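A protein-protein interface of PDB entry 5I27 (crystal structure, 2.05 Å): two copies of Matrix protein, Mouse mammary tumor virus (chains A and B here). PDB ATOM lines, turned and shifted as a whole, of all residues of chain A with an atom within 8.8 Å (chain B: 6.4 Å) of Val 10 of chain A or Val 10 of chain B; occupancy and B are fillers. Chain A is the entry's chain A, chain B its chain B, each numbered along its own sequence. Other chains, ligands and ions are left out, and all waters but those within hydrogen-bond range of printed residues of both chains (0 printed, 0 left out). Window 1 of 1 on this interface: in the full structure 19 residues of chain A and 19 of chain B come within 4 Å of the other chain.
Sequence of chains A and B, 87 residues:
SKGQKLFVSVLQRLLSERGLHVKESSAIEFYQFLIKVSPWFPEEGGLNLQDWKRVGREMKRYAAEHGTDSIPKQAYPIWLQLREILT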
ATOM      1  N   GLY A   3      -6.468 -32.968  12.765  1.00  0.00           N
ATOM      2  CA  GLY A   3      -6.286 -32.609  14.174  1.00  0.00           C
ATOM      3  C   GLY A   3      -6.122 -31.108  14.289  1.00  0.00           C
ATOM      4  O   GLY A   3      -6.196 -30.562  15.386  1.00  0.00           O
ATOM      5  N   GLN A   4      -5.917 -30.459  13.136  1.00  0.00           N
ATOM      6  CA  GLN A   4      -5.745 -28.988  13.016  1.00  0.00           C
ATOM      7  C   GLN A   4      -6.914 -28.164  13.549  1.00  0.00           C
ATOM      8  O   GLN A   4      -6.787 -27.467  14.554  1.00  0.00           O
ATOM      9  CB  GLN A   4      -5.502 -28.609  11.551  1.00  0.00           C
ATOM     10  CG  GLN A   4      -5.084 -27.173  11.297  1.00  0.00           C
ATOM     11  CD  GLN A   4      -4.617 -26.975   9.867  1.00  0.00           C
ATOM     12  OE1 GLN A   4      -3.545 -27.465   9.478  1.00  0.00           O
ATOM     13  NE2 GLN A   4      -5.427 -26.264   9.060  1.00  0.00           N
ATOM     14  N   LYS A   5      -8.054 -28.241  12.864  1.00  0.00           N
ATOM     15  CA  LYS A   5      -9.204 -27.418  13.232  1.00  0.00           C
ATOM     16  C   LYS A   5      -9.516 -27.537  14.735  1.00  0.00           C
ATOM     17  O   LYS A   5      -9.867 -26.574  15.364  1.00  0.00           O
ATOM     18  CB  LYS A   5     -10.448 -27.783  12.402  1.00  0.00           C
ATOM     19  CG  LYS A   5     -11.551 -26.756  12.570  1.00  0.00           C
ATOM     20  CD  LYS A   5     -12.853 -27.254  12.009  1.00  0.00           C
ATOM     21  CE  LYS A   5     -13.897 -26.166  12.068  1.00  0.00           C
ATOM     22  NZ  LYS A   5     -15.229 -26.802  12.006  1.00  0.00           N
ATOM     23  N   LEU A   6      -9.379 -28.728  15.301  1.00  0.00           N
ATOM     24  CA  LEU A   6      -9.529 -28.890  16.753  1.00  0.00           C
ATOM     25  C   LEU A   6      -8.506 -28.093  17.552  1.00  0.00           C
ATOM     26  O   LEU A   6      -8.874 -27.293  18.432  1.00  0.00           O
ATOM     27  CB  LEU A   6      -9.426 -30.359  17.154  1.00  0.00           C
ATOM     28  CG  LEU A   6      -9.776 -30.661  18.612  1.00  0.00           C
ATOM     29  CD1 LEU A   6     -11.041 -29.909  19.033  1.00  0.00           C
ATOM     30  CD2 LEU A   6      -9.927 -32.160  18.801  1.00  0.00           C
ATOM     31  N   PHE A   7      -7.217 -28.316  17.265  1.00  0.00           N
ATOM     32  CA  PHE A   7      -6.192 -27.617  18.033  1.00  0.00           C
ATOM     33  C   PHE A   7      -6.334 -26.104  17.872  1.00  0.00           C
ATOM     34  O   PHE A   7      -6.220 -25.346  18.834  1.00  0.00           O
ATOM     35  CB  PHE A   7      -4.780 -27.991  17.590  1.00  0.00           C
ATOM     36  CG  PHE A   7      -3.719 -27.317  18.411  1.00  0.00           C
ATOM     37  CD1 PHE A   7      -3.248 -26.060  18.064  1.00  0.00           C
ATOM     38  CD2 PHE A   7      -3.266 -27.906  19.575  1.00  0.00           C
ATOM     39  CE1 PHE A   7      -2.285 -25.426  18.832  1.00  0.00           C
ATOM     40  CE2 PHE A   7      -2.294 -27.292  20.357  1.00  0.00           C
ATOM     41  CZ  PHE A   7      -1.802 -26.049  19.986  1.00  0.00           C
ATOM     42  N   VAL A   8      -6.595 -25.687  16.651  1.00  0.00           N
ATOM     43  CA  VAL A   8      -6.744 -24.283  16.363  1.00  0.00           C
ATOM     44  C   VAL A   8      -7.901 -23.678  17.150  1.00  0.00           C
ATOM     45  O   VAL A   8      -7.805 -22.533  17.602  1.00  0.00           O
ATOM     46  CB  VAL A   8      -6.924 -24.032  14.863  1.00  0.00           C
ATOM     47  CG1 VAL A   8      -7.605 -22.671  14.593  1.00  0.00           C
ATOM     48  CG2 VAL A   8      -5.561 -24.113  14.197  1.00  0.00           C
ATOM     49  N   SER A   9      -8.973 -24.454  17.340  1.00  0.00           N
ATOM     50  CA  SER A   9     -10.151 -23.943  18.040  1.00  0.00           C
ATOM     51  C   SER A   9      -9.849 -23.801  19.526  1.00  0.00           C
ATOM     52  O   SER A   9     -10.288 -22.828  20.182  1.00  0.00           O
ATOM     53  CB  SER A   9     -11.380 -24.830  17.755  1.00  0.00           C
ATOM     54  OG  SER A   9     -11.320 -26.039  18.516  1.00  0.00           O
ATOM     55  N   VAL A  10      -9.036 -24.704  20.058  1.00  0.00           N
ATOM     56  CA  VAL A  10      -8.615 -24.596  21.477  1.00  0.00           C
ATOM     57  C   VAL A  10      -7.716 -23.405  21.725  1.00  0.00           C
ATOM     58  O   VAL A  10      -7.881 -22.617  22.669  1.00  0.00           O
ATOM     59  CB  VAL A  10      -7.847 -25.848  21.913  1.00  0.00           C
ATOM     60  CG1 VAL A  10      -7.247 -25.635  23.294  1.00  0.00           C
ATOM     61  CG2 VAL A  10      -8.799 -27.039  21.912  1.00  0.00           C
ATOM     62  N   LEU A  11      -6.725 -23.286  20.866  1.00  0.00           N
ATOM     63  CA  LEU A  11      -5.822 -22.165  20.932  1.00  0.00           C
ATOM     64  C   LEU A  11      -6.533 -20.790  20.931  1.00  0.00           C
ATOM     65  O   LEU A  11      -6.264 -19.927  21.783  1.00  0.00           O
ATOM     66  CB  LEU A  11      -4.903 -22.264  19.716  1.00  0.00           C
ATOM     67  CG  LEU A  11      -3.932 -21.111  19.671  1.00  0.00           C
ATOM     68  CD1 LEU A  11      -2.806 -21.466  20.620  1.00  0.00           C
ATOM     69  CD2 LEU A  11      -3.402 -20.868  18.268  1.00  0.00           C
ATOM     70  N   GLN A  12      -7.427 -20.579  19.963  1.00  0.00           N
ATOM     71  CA  GLN A  12      -8.143 -19.299  19.844  1.00  0.00           C
ATOM     72  C   GLN A  12      -8.990 -19.009  21.093  1.00  0.00           C
ATOM     73  O   GLN A  12      -9.060 -17.863  21.601  1.00  0.00           O
ATOM     74  CB  GLN A  12      -9.000 -19.298  18.557  1.00  0.00           C
ATOM     75  CG  GLN A  12      -8.145 -19.049  17.298  1.00  0.00           C
ATOM     76  CD  GLN A  12      -8.921 -18.970  15.985  1.00  0.00           C
ATOM     77  OE1 GLN A  12      -9.891 -19.700  15.764  1.00  0.00           O
ATOM     78  NE2 GLN A  12      -8.470 -18.101  15.088  1.00  0.00           N
ATOM     79  N   ARG A  13      -9.636 -20.045  21.598  1.00  0.00           N
ATOM     80  CA  ARG A  13     -10.475 -19.904  22.790  1.00  0.00           C
ATOM     81  C   ARG A  13      -9.615 -19.541  23.995  1.00  0.00           C
ATOM     82  O   ARG A  13      -9.919 -18.580  24.685  1.00  0.00           O
ATOM     83  CB  ARG A  13     -11.276 -21.185  23.049  1.00  0.00           C
ATOM     84  CG  ARG A  13     -12.093 -21.125  24.333  1.00  0.00           C
ATOM     85  CD  ARG A  13     -13.185 -22.187  24.416  1.00  0.00           C
ATOM     86  NE  ARG A  13     -14.259 -21.651  25.255  1.00  0.00           N
ATOM     87  CZ  ARG A  13     -15.346 -21.034  24.790  1.00  0.00           C
ATOM     88  NH1 ARG A  13     -15.555 -20.935  23.487  1.00  0.00           N
ATOM     89  NH2 ARG A  13     -16.246 -20.539  25.637  1.00  0.00           N
ATOM     90  N   LEU A  14      -8.519 -20.270  24.209  1.00  0.00           N
ATOM     91  CA  LEU A  14      -7.627 -20.019  25.344  1.00  0.00           C
ATOM     92  C   LEU A  14      -7.055 -18.597  25.334  1.00  0.00           C
ATOM     93  O   LEU A  14      -7.075 -17.913  26.358  1.00  0.00           O
ATOM     94  CB  LEU A  14      -6.463 -21.046  25.415  1.00  0.00           C
ATOM     95  CG  LEU A  14      -6.761 -22.521  25.687  1.00  0.00           C
ATOM     96  CD1 LEU A  14      -5.478 -23.293  25.494  1.00  0.00           C
ATOM     97  CD2 LEU A  14      -7.289 -22.743  27.087  1.00  0.00           C
ATOM     98  N   LEU A  15      -6.538 -18.170  24.190  1.00  0.00           N
ATOM     99  CA  LEU A  15      -6.007 -16.819  24.059  1.00  0.00           C
ATOM    100  C   LEU A  15      -7.114 -15.770  24.174  1.00  0.00           C
ATOM    101  O   LEU A  15      -6.902 -14.752  24.822  1.00  0.00           O
ATOM    102  CB  LEU A  15      -5.190 -16.640  22.772  1.00  0.00           C
ATOM    103  CG  LEU A  15      -4.039 -17.635  22.647  1.00  0.00           C
ATOM    104  CD1 LEU A  15      -3.320 -17.505  21.309  1.00  0.00           C
ATOM    105  CD2 LEU A  15      -3.080 -17.437  23.802  1.00  0.00           C
ATOM    106  N   SER A  16      -8.285 -16.042  23.596  1.00  0.00           N
ATOM    107  CA  SER A  16      -9.421 -15.096  23.621  1.00  0.00           C
ATOM    108  C   SER A  16      -9.622 -14.646  25.024  1.00  0.00           C
ATOM    109  O   SER A  16      -9.600 -13.452  25.318  1.00  0.00           O
ATOM    110  CB  SER A  16     -10.734 -15.760  23.230  1.00  0.00           C
ATOM    111  OG  SER A  16     -10.954 -15.662  21.855  1.00  0.00           O
ATOM    112  N   GLU A  17      -9.806 -15.634  25.889  1.00  0.00           N
ATOM    113  CA  GLU A  17     -10.111 -15.412  27.275  1.00  0.00           C
ATOM    114  C   GLU A  17      -9.076 -14.584  28.019  1.00  0.00           C
ATOM    115  O   GLU A  17      -9.365 -14.122  29.100  1.00  0.00           O
ATOM    116  CB  GLU A  17     -10.336 -16.742  27.977  1.00  0.00           C
ATOM    117  CG  GLU A  17     -11.640 -17.420  27.567  1.00  0.00           C
ATOM    118  CD  GLU A  17     -11.755 -18.849  28.096  1.00  0.00           C
ATOM    119  OE1 GLU A  17     -10.711 -19.547  28.190  1.00  0.00           O
ATOM    120  OE2 GLU A  17     -12.890 -19.279  28.417  1.00  0.00           O
ATOM    121  N   ARG A  18      -7.881 -14.397  27.458  1.00  0.00           N
ATOM    122  CA  ARG A  18      -6.861 -13.543  28.071  1.00  0.00           C
ATOM    123  C   ARG A  18      -6.753 -12.206  27.318  1.00  0.00           C
ATOM    124  O   ARG A  18      -5.832 -11.423  27.554  1.00  0.00           O
ATOM    125  CB  ARG A  18      -5.493 -14.261  28.142  1.00  0.00           C
ATOM    126  CG  ARG A  18      -5.347 -15.288  29.273  1.00  0.00           C
ATOM    127  CD  ARG A  18      -6.086 -16.601  28.992  1.00  0.00           C
ATOM    128  NE  ARG A  18      -6.026 -17.540  30.110  1.00  0.00           N
ATOM    129  CZ  ARG A  18      -6.694 -18.685  30.163  1.00  0.00           C
ATOM    130  NH1 ARG A  18      -7.479 -19.056  29.159  1.00  0.00           N
ATOM    131  NH2 ARG A  18      -6.579 -19.459  31.222  1.00  0.00           N
ATOM    132  N   ALA A  27      -2.881 -18.901  13.221  1.00  0.00           N
ATOM    133  CA  ALA A  27      -3.010 -20.092  14.088  1.00  0.00           C
ATOM    134  C   ALA A  27      -2.801 -21.414  13.348  1.00  0.00           C
ATOM    135  O   ALA A  27      -2.209 -22.374  13.903  1.00  0.00           O
ATOM    136  CB  ALA A  27      -4.354 -20.093  14.801  1.00  0.00           C
ATOM    137  N   PHE A  41       3.402 -34.923  18.952  1.00  0.00           N
ATOM    138  CA  PHE A  41       2.371 -34.129  19.665  1.00  0.00           C
ATOM    139  C   PHE A  41       0.888 -34.507  19.393  1.00  0.00           C
ATOM    140  O   PHE A  41       0.141 -34.725  20.347  1.00  0.00           O
ATOM    141  CB  PHE A  41       2.617 -32.595  19.591  1.00  0.00           C
ATOM    142  CG  PHE A  41       1.813 -31.806  20.614  1.00  0.00           C
ATOM    143  CD1 PHE A  41       0.522 -31.368  20.323  1.00  0.00           C
ATOM    144  CD2 PHE A  41       2.324 -31.544  21.874  1.00  0.00           C
ATOM    145  CE1 PHE A  41      -0.227 -30.670  21.261  1.00  0.00           C
ATOM    146  CE2 PHE A  41       1.568 -30.850  22.826  1.00  0.00           C
ATOM    147  CZ  PHE A  41       0.299 -30.417  22.507  1.00  0.00           C
ATOM    148  N   GLY A  45       0.636 -36.264  22.704  1.00  0.00           N
ATOM    149  CA  GLY A  45       0.782 -35.065  23.526  1.00  0.00           C
ATOM    150  C   GLY A  45      -0.498 -34.479  24.093  1.00  0.00           C
ATOM    151  O   GLY A  45      -1.548 -34.561  23.468  1.00  0.00           O
ATOM    152  N   GLY A  46      -0.392 -33.875  25.278  1.00  0.00           N
ATOM    153  CA  GLY A  46      -1.505 -33.198  25.890  1.00  0.00           C
ATOM    154  C   GLY A  46      -1.197 -31.728  26.063  1.00  0.00           C
ATOM    155  O   GLY A  46      -0.035 -31.337  26.170  1.00  0.00           O
ATOM    156  N   LEU A  47      -2.239 -30.910  26.111  1.00  0.00           N
ATOM    157  CA  LEU A  47      -2.090 -29.526  26.540  1.00  0.00           C
ATOM    158  C   LEU A  47      -1.794 -29.465  28.043  1.00  0.00           C
ATOM    159  O   LEU A  47      -2.646 -29.100  28.848  1.00  0.00           O
ATOM    160  CB  LEU A  47      -3.369 -28.767  26.220  1.00  0.00           C
ATOM    161  CG  LEU A  47      -3.313 -27.290  25.860  1.00  0.00           C
ATOM    162  CD1 LEU A  47      -2.407 -27.018  24.665  1.00  0.00           C
ATOM    163  CD2 LEU A  47      -4.733 -26.845  25.565  1.00  0.00           C
ATOM    164  N   ASN A  48      -0.579 -29.843  28.402  1.00  0.00           N
ATOM    165  CA  ASN A  48      -0.093 -29.872  29.784  1.00  0.00           C
ATOM    166  C   ASN A  48       1.352 -29.335  29.815  1.00  0.00           C
ATOM    167  O   ASN A  48       2.022 -29.348  28.797  1.00  0.00           O
ATOM    168  CB  ASN A  48      -0.164 -31.307  30.357  1.00  0.00           C
ATOM    169  CG  ASN A  48       0.866 -32.268  29.739  1.00  0.00           C
ATOM    170  OD1 ASN A  48       2.082 -32.045  29.814  1.00  0.00           O
ATOM    171  ND2 ASN A  48       0.383 -33.369  29.168  1.00  0.00           N
ATOM    172  N   LEU A  82       0.675 -19.586  25.641  1.00  0.00           N
ATOM    173  CA  LEU A  82       0.087 -20.842  26.093  1.00  0.00           C
ATOM    174  C   LEU A  82       0.862 -21.463  27.251  1.00  0.00           C
ATOM    175  O   LEU A  82       0.227 -21.977  28.171  1.00  0.00           O
ATOM    176  CB  LEU A  82      -0.135 -21.849  24.955  1.00  0.00           C
ATOM    177  CG  LEU A  82      -1.092 -21.375  23.856  1.00  0.00           C
ATOM    178  CD1 LEU A  82      -1.121 -22.534  22.871  1.00  0.00           C
ATOM    179  CD2 LEU A  82      -2.503 -21.123  24.362  1.00  0.00           C
ATOM    180  N   ILE A  85      -0.587 -19.832  30.330  1.00  0.00           N
ATOM    181  CA  ILE A  85      -1.921 -20.360  30.616  1.00  0.00           C
ATOM    182  C   ILE A  85      -1.835 -21.708  31.308  1.00  0.00           C
ATOM    183  O   ILE A  85      -2.654 -22.016  32.160  1.00  0.00           O
ATOM    184  CB  ILE A  85      -2.763 -20.501  29.341  1.00  0.00           C
ATOM    185  CG1 ILE A  85      -3.061 -19.115  28.754  1.00  0.00           C
ATOM    186  CG2 ILE A  85      -4.077 -21.216  29.618  1.00  0.00           C
ATOM    187  CD1 ILE A  85      -3.131 -19.098  27.240  1.00  0.00           C
ATOM    188  N   LEU A  86      -0.830 -22.498  30.949  1.00  0.00           N
ATOM    189  CA  LEU A  86      -0.671 -23.828  31.541  1.00  0.00           C
ATOM    190  C   LEU A  86      -0.053 -23.812  32.947  1.00  0.00           C
ATOM    191  O   LEU A  86       0.419 -24.843  33.429  1.00  0.00           O
ATOM    192  CB  LEU A  86       0.080 -24.774  30.584  1.00  0.00           C
ATOM    193  CG  LEU A  86      -0.538 -25.001  29.190  1.00  0.00           C
ATOM    194  CD1 LEU A  86       0.371 -25.865  28.310  1.00  0.00           C
ATOM    195  CD2 LEU A  86      -1.959 -25.565  29.188  1.00  0.00           C
ATOM    196  N   LYS B   5      -5.318 -37.858  24.295  1.00  0.00           N
ATOM    197  CA  LYS B   5      -4.647 -37.131  25.376  1.00  0.00           C
ATOM    198  C   LYS B   5      -4.984 -35.637  25.286  1.00  0.00           C
ATOM    199  O   LYS B   5      -5.375 -35.020  26.295  1.00  0.00           O
ATOM    200  CB  LYS B   5      -3.121 -37.394  25.386  1.00  0.00           C
ATOM    201  CG  LYS B   5      -2.472 -37.087  26.748  1.00  0.00           C
ATOM    202  CD  LYS B   5      -1.016 -37.537  26.821  1.00  0.00           C
ATOM    203  CE  LYS B   5      -0.532 -37.486  28.261  1.00  0.00           C
ATOM    204  NZ  LYS B   5       0.890 -37.049  28.347  1.00  0.00           N
ATOM    205  N   LEU B   6      -4.863 -35.087  24.068  1.00  0.00           N
ATOM    206  CA  LEU B   6      -5.150 -33.699  23.813  1.00  0.00           C
ATOM    207  C   LEU B   6      -6.557 -33.337  24.164  1.00  0.00           C
ATOM    208  O   LEU B   6      -6.797 -32.413  24.939  1.00  0.00           O
ATOM    209  CB  LEU B   6      -4.911 -33.319  22.340  1.00  0.00           C
ATOM    210  CG  LEU B   6      -5.338 -31.851  22.195  1.00  0.00           C
ATOM    211  CD1 LEU B   6      -4.165 -30.966  22.578  1.00  0.00           C
ATOM    212  CD2 LEU B   6      -5.921 -31.478  20.825  1.00  0.00           C
ATOM    213  N   PHE B   7      -7.514 -34.045  23.561  1.00  0.00           N
ATOM    214  CA  PHE B   7      -8.910 -33.771  23.874  1.00  0.00           C
ATOM    215  C   PHE B   7      -9.244 -33.845  25.373  1.00  0.00           C
ATOM    216  O   PHE B   7      -9.930 -32.963  25.900  1.00  0.00           O
ATOM    217  CB  PHE B   7      -9.853 -34.673  23.075  1.00  0.00           C
ATOM    218  CG  PHE B   7     -11.294 -34.354  23.295  1.00  0.00           C
ATOM    219  CD1 PHE B   7     -12.014 -34.987  24.311  1.00  0.00           C
ATOM    220  CD2 PHE B   7     -11.928 -33.387  22.528  1.00  0.00           C
ATOM    221  CE1 PHE B   7     -13.353 -34.677  24.523  1.00  0.00           C
ATOM    222  CE2 PHE B   7     -13.261 -33.053  22.750  1.00  0.00           C
ATOM    223  CZ  PHE B   7     -13.977 -33.699  23.749  1.00  0.00           C
ATOM    224  N   VAL B   8      -8.782 -34.898  26.042  1.00  0.00           N
ATOM    225  CA  VAL B   8      -9.031 -35.086  27.487  1.00  0.00           C
ATOM    226  C   VAL B   8      -8.436 -33.933  28.277  1.00  0.00           C
ATOM    227  O   VAL B   8      -9.086 -33.396  29.199  1.00  0.00           O
ATOM    228  CB  VAL B   8      -8.467 -36.441  27.998  1.00  0.00           C
ATOM    229  CG1 VAL B   8      -8.316 -36.474  29.520  1.00  0.00           C
ATOM    230  CG2 VAL B   8      -9.349 -37.616  27.555  1.00  0.00           C
ATOM    231  N   SER B   9      -7.207 -33.534  27.931  1.00  0.00           N
ATOM    232  CA  SER B   9      -6.548 -32.447  28.652  1.00  0.00           C
ATOM    233  C   SER B   9      -7.378 -31.175  28.474  1.00  0.00           C
ATOM    234  O   SER B   9      -7.591 -30.395  29.419  1.00  0.00           O
ATOM    235  CB  SER B   9      -5.098 -32.293  28.167  1.00  0.00           C
ATOM    236  OG  SER B   9      -5.058 -31.617  26.916  1.00  0.00           O
ATOM    237  N   VAL B  10      -7.937 -31.000  27.279  1.00  0.00           N
ATOM    238  CA  VAL B  10      -8.813 -29.845  27.019  1.00  0.00           C
ATOM    239  C   VAL B  10     -10.153 -29.879  27.776  1.00  0.00           C
ATOM    240  O   VAL B  10     -10.591 -28.882  28.422  1.00  0.00           O
ATOM    241  CB  VAL B  10      -9.021 -29.650  25.491  1.00  0.00           C
ATOM    242  CG1 VAL B  10     -10.021 -28.548  25.194  1.00  0.00           C
ATOM    243  CG2 VAL B  10      -7.702 -29.338  24.813  1.00  0.00           C
ATOM    244  N   LEU B  11     -10.798 -31.029  27.738  1.00  0.00           N
ATOM    245  CA  LEU B  11     -12.056 -31.208  28.441  1.00  0.00           C
ATOM    246  C   LEU B  11     -11.954 -30.892  29.935  1.00  0.00           C
ATOM    247  O   LEU B  11     -12.795 -30.190  30.519  1.00  0.00           O
ATOM    248  CB  LEU B  11     -12.489 -32.657  28.267  1.00  0.00           C
ATOM    249  CG  LEU B  11     -13.744 -33.148  28.970  1.00  0.00           C
ATOM    250  CD1 LEU B  11     -14.960 -32.251  28.676  1.00  0.00           C
ATOM    251  CD2 LEU B  11     -13.974 -34.538  28.414  1.00  0.00           C
ATOM    252  N   GLN B  12     -10.935 -31.456  30.562  1.00  0.00           N
ATOM    253  CA  GLN B  12     -10.801 -31.360  31.989  1.00  0.00           C
ATOM    254  C   GLN B  12     -10.520 -29.927  32.386  1.00  0.00           C
ATOM    255  O   GLN B  12     -11.131 -29.446  33.330  1.00  0.00           O
ATOM    256  CB  GLN B  12      -9.710 -32.292  32.446  1.00  0.00           C
ATOM    257  CG  GLN B  12     -10.101 -33.715  32.136  1.00  0.00           C
ATOM    258  CD  GLN B  12      -9.263 -34.669  32.894  1.00  0.00           C
ATOM    259  OE1 GLN B  12      -8.031 -34.577  32.849  1.00  0.00           O
ATOM    260  NE2 GLN B  12      -9.908 -35.587  33.626  1.00  0.00           N
ATOM    261  N   ARG B  13      -9.644 -29.241  31.644  1.00  0.00           N
ATOM    262  CA  ARG B  13      -9.492 -27.777  31.801  1.00  0.00           C
ATOM    263  C   ARG B  13     -10.852 -27.014  31.679  1.00  0.00           C
ATOM    264  O   ARG B  13     -11.262 -26.286  32.598  1.00  0.00           O
ATOM    265  CB  ARG B  13      -8.405 -27.240  30.842  1.00  0.00           C
ATOM    266  CG  ARG B  13      -8.221 -25.730  30.802  1.00  0.00           C
ATOM    267  CD  ARG B  13      -6.998 -25.325  29.971  1.00  0.00           C
ATOM    268  NE  ARG B  13      -5.796 -25.929  30.548  1.00  0.00           N
ATOM    269  CZ  ARG B  13      -5.028 -25.335  31.460  1.00  0.00           C
ATOM    270  NH1 ARG B  13      -5.306 -24.101  31.871  1.00  0.00           N
ATOM    271  NH2 ARG B  13      -3.974 -25.968  31.950  1.00  0.00           N
ATOM    272  N   LEU B  14     -11.569 -27.203  30.571  1.00  0.00           N
ATOM    273  CA  LEU B  14     -12.828 -26.496  30.378  1.00  0.00           C
ATOM    274  C   LEU B  14     -13.817 -26.748  31.474  1.00  0.00           C
ATOM    275  O   LEU B  14     -14.508 -25.838  31.904  1.00  0.00           O
ATOM    276  CB  LEU B  14     -13.496 -26.889  29.062  1.00  0.00           C
ATOM    277  CG  LEU B  14     -12.942 -26.346  27.765  1.00  0.00           C
ATOM    278  CD1 LEU B  14     -13.470 -27.248  26.667  1.00  0.00           C
ATOM    279  CD2 LEU B  14     -13.405 -24.915  27.615  1.00  0.00           C
ATOM    280  N   LEU B  15     -13.918 -27.992  31.915  1.00  0.00           N
ATOM    281  CA  LEU B  15     -14.850 -28.292  32.968  1.00  0.00           C
ATOM    282  C   LEU B  15     -14.380 -27.782  34.320  1.00  0.00           C
ATOM    283  O   LEU B  15     -15.201 -27.303  35.103  1.00  0.00           O
ATOM    284  CB  LEU B  15     -15.141 -29.780  33.042  1.00  0.00           C
ATOM    285  CG  LEU B  15     -15.981 -30.395  31.918  1.00  0.00           C
ATOM    286  CD1 LEU B  15     -16.169 -31.877  32.187  1.00  0.00           C
ATOM    287  CD2 LEU B  15     -17.331 -29.707  31.781  1.00  0.00           C
ATOM    288  N   LEU B  47     -13.823 -27.303  18.506  1.00  0.00           N
ATOM    289  CA  LEU B  47     -14.622 -26.800  19.628  1.00  0.00           C
ATOM    290  C   LEU B  47     -15.434 -25.582  19.224  1.00  0.00           C
ATOM    291  O   LEU B  47     -15.093 -24.451  19.551  1.00  0.00           O
ATOM    292  CB  LEU B  47     -13.696 -26.423  20.774  1.00  0.00           C
ATOM    293  CG  LEU B  47     -13.556 -27.374  21.959  1.00  0.00           C
ATOM    294  CD1 LEU B  47     -13.673 -28.839  21.566  1.00  0.00           C
ATOM    295  CD2 LEU B  47     -12.208 -27.074  22.589  1.00  0.00           C
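Hydrophobic or aromatic side chains of chain B that line the printed part of chain A: Leu 6, Val 10 and Leu 47.
Among the printed residues, no Asp or Glu carboxylate lies within 4 Å of a Lys or Arg side-chain nitrogen of the other chain.
Of chain A, only Val 10 and Leu 47 come within 4 Å of Val 10 of chain B.
Of chain A, only Gly 46 and Leu 47 come within 4 Å of Ser 9 of chain B.
Of the printed residues of chain A, Leu 47 of chain B touches Leu 6 (3.8 Å), Ser 9 (2.8 Å) and Val 10 (3.5 Å).
Printed residues of chain B within 4 Å of Asn 48 of chain A: Lys 5 (3.8 Å).
Printed residues of chain B within 4 Å of Gly 46 of chain A: Ser 9.
Of the printed residues of chain B, Leu 14 of chain A touches Arg 13 (3.9 Å).
The nearest residue of chain B that does not touch Val 10 of chain A is Leu 6 of chain B (5.4 Å).
The nearest residue of chain A that does not touch Val 10 of chain B is Leu 6 of chain A (6.4 Å).
Leu 6 of chain A touches Leu 47 of chain B, but with the chains exchanged Leu 47 of chain A does not touch Leu 6 of chain B (4.02 Å).
Ser 9 of chain A touches Leu 47 of chain B, and with the chains exchanged Leu 47 of chain A touches Ser 9 of chain B.
Val 10 of chain B touches its own counterpart, Val 10 of chain A.
Leu 14 of chain A touches Arg 13 of chain B, but with the chains exchanged Arg 13 of chain A does not touch Leu 14 of chain B (4.1 Å).
Of the 13 pairs that touch across the chains among the printed residues, 5 have their exchanged pair printed and touching as well.
Among the printed residues, pairs that only touch across the chains: Leu 86 of chain A with Arg 13 of chain B (3.4 Å), Val 10 of chain A with Leu 47 of chain B (3.5 Å), Gly 45 of chain A with Lys 5 of chain B (3.8 Å), Asn 48 of chain A with Lys 5 of chain B (3.8 Å), Leu 6 of chain A with Leu 47 of chain B (3.8 Å), Val 10 of chain A with Val 10 of chain B (3.8 Å), Leu 14 of chain A with Arg 13 of chain B (3.9 Å), Leu 47 of chain A with Val 10 of chain B (3.9 Å) and Gly 46 of chain A with Ser 9 of chain B (3.96 Å).
O of Lys 5 of chain B lies close to OG of Ser 9 of chain B.
The side-chain hydroxyl (OG) of Ser 9 of chain B lies within hydrogen-bond range of the backbone carbonyl oxygen (O) of Leu 6 of chain B (2.8 Å).
The backbone carbonyl oxygen of Leu 14 of chain A is in hydrogen-bond range of the guanidinium group of Arg 18 of chain A, at 3.1 Å.
The backbone carbonyl oxygen (O) of Leu 6 of chain A lies within hydrogen-bond range of the side-chain hydroxyl (OG) of Ser 9 of chain A, 2.7 Å away.
The backbone NH (N) of Leu 6 of chain B is in hydrogen-bond range of the backbone carbonyl oxygen (O) of Gly 45 of chain A, at 3.4 Å.
The side-chain hydroxyl (OG) of Ser 9 of chain A is in hydrogen-bond range of the backbone NH (N) of Leu 47 of chain B (2.8 Å).
OG of Ser 9 of chain B is in hydrogen-bond range of N of Leu 47 of chain A (3.0 Å).
The backbone carbonyl oxygen of Ile 85 of chain A sits at hydrogen-bond distance from the guanidinium group of Arg 13 of chain B (3.4 Å).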
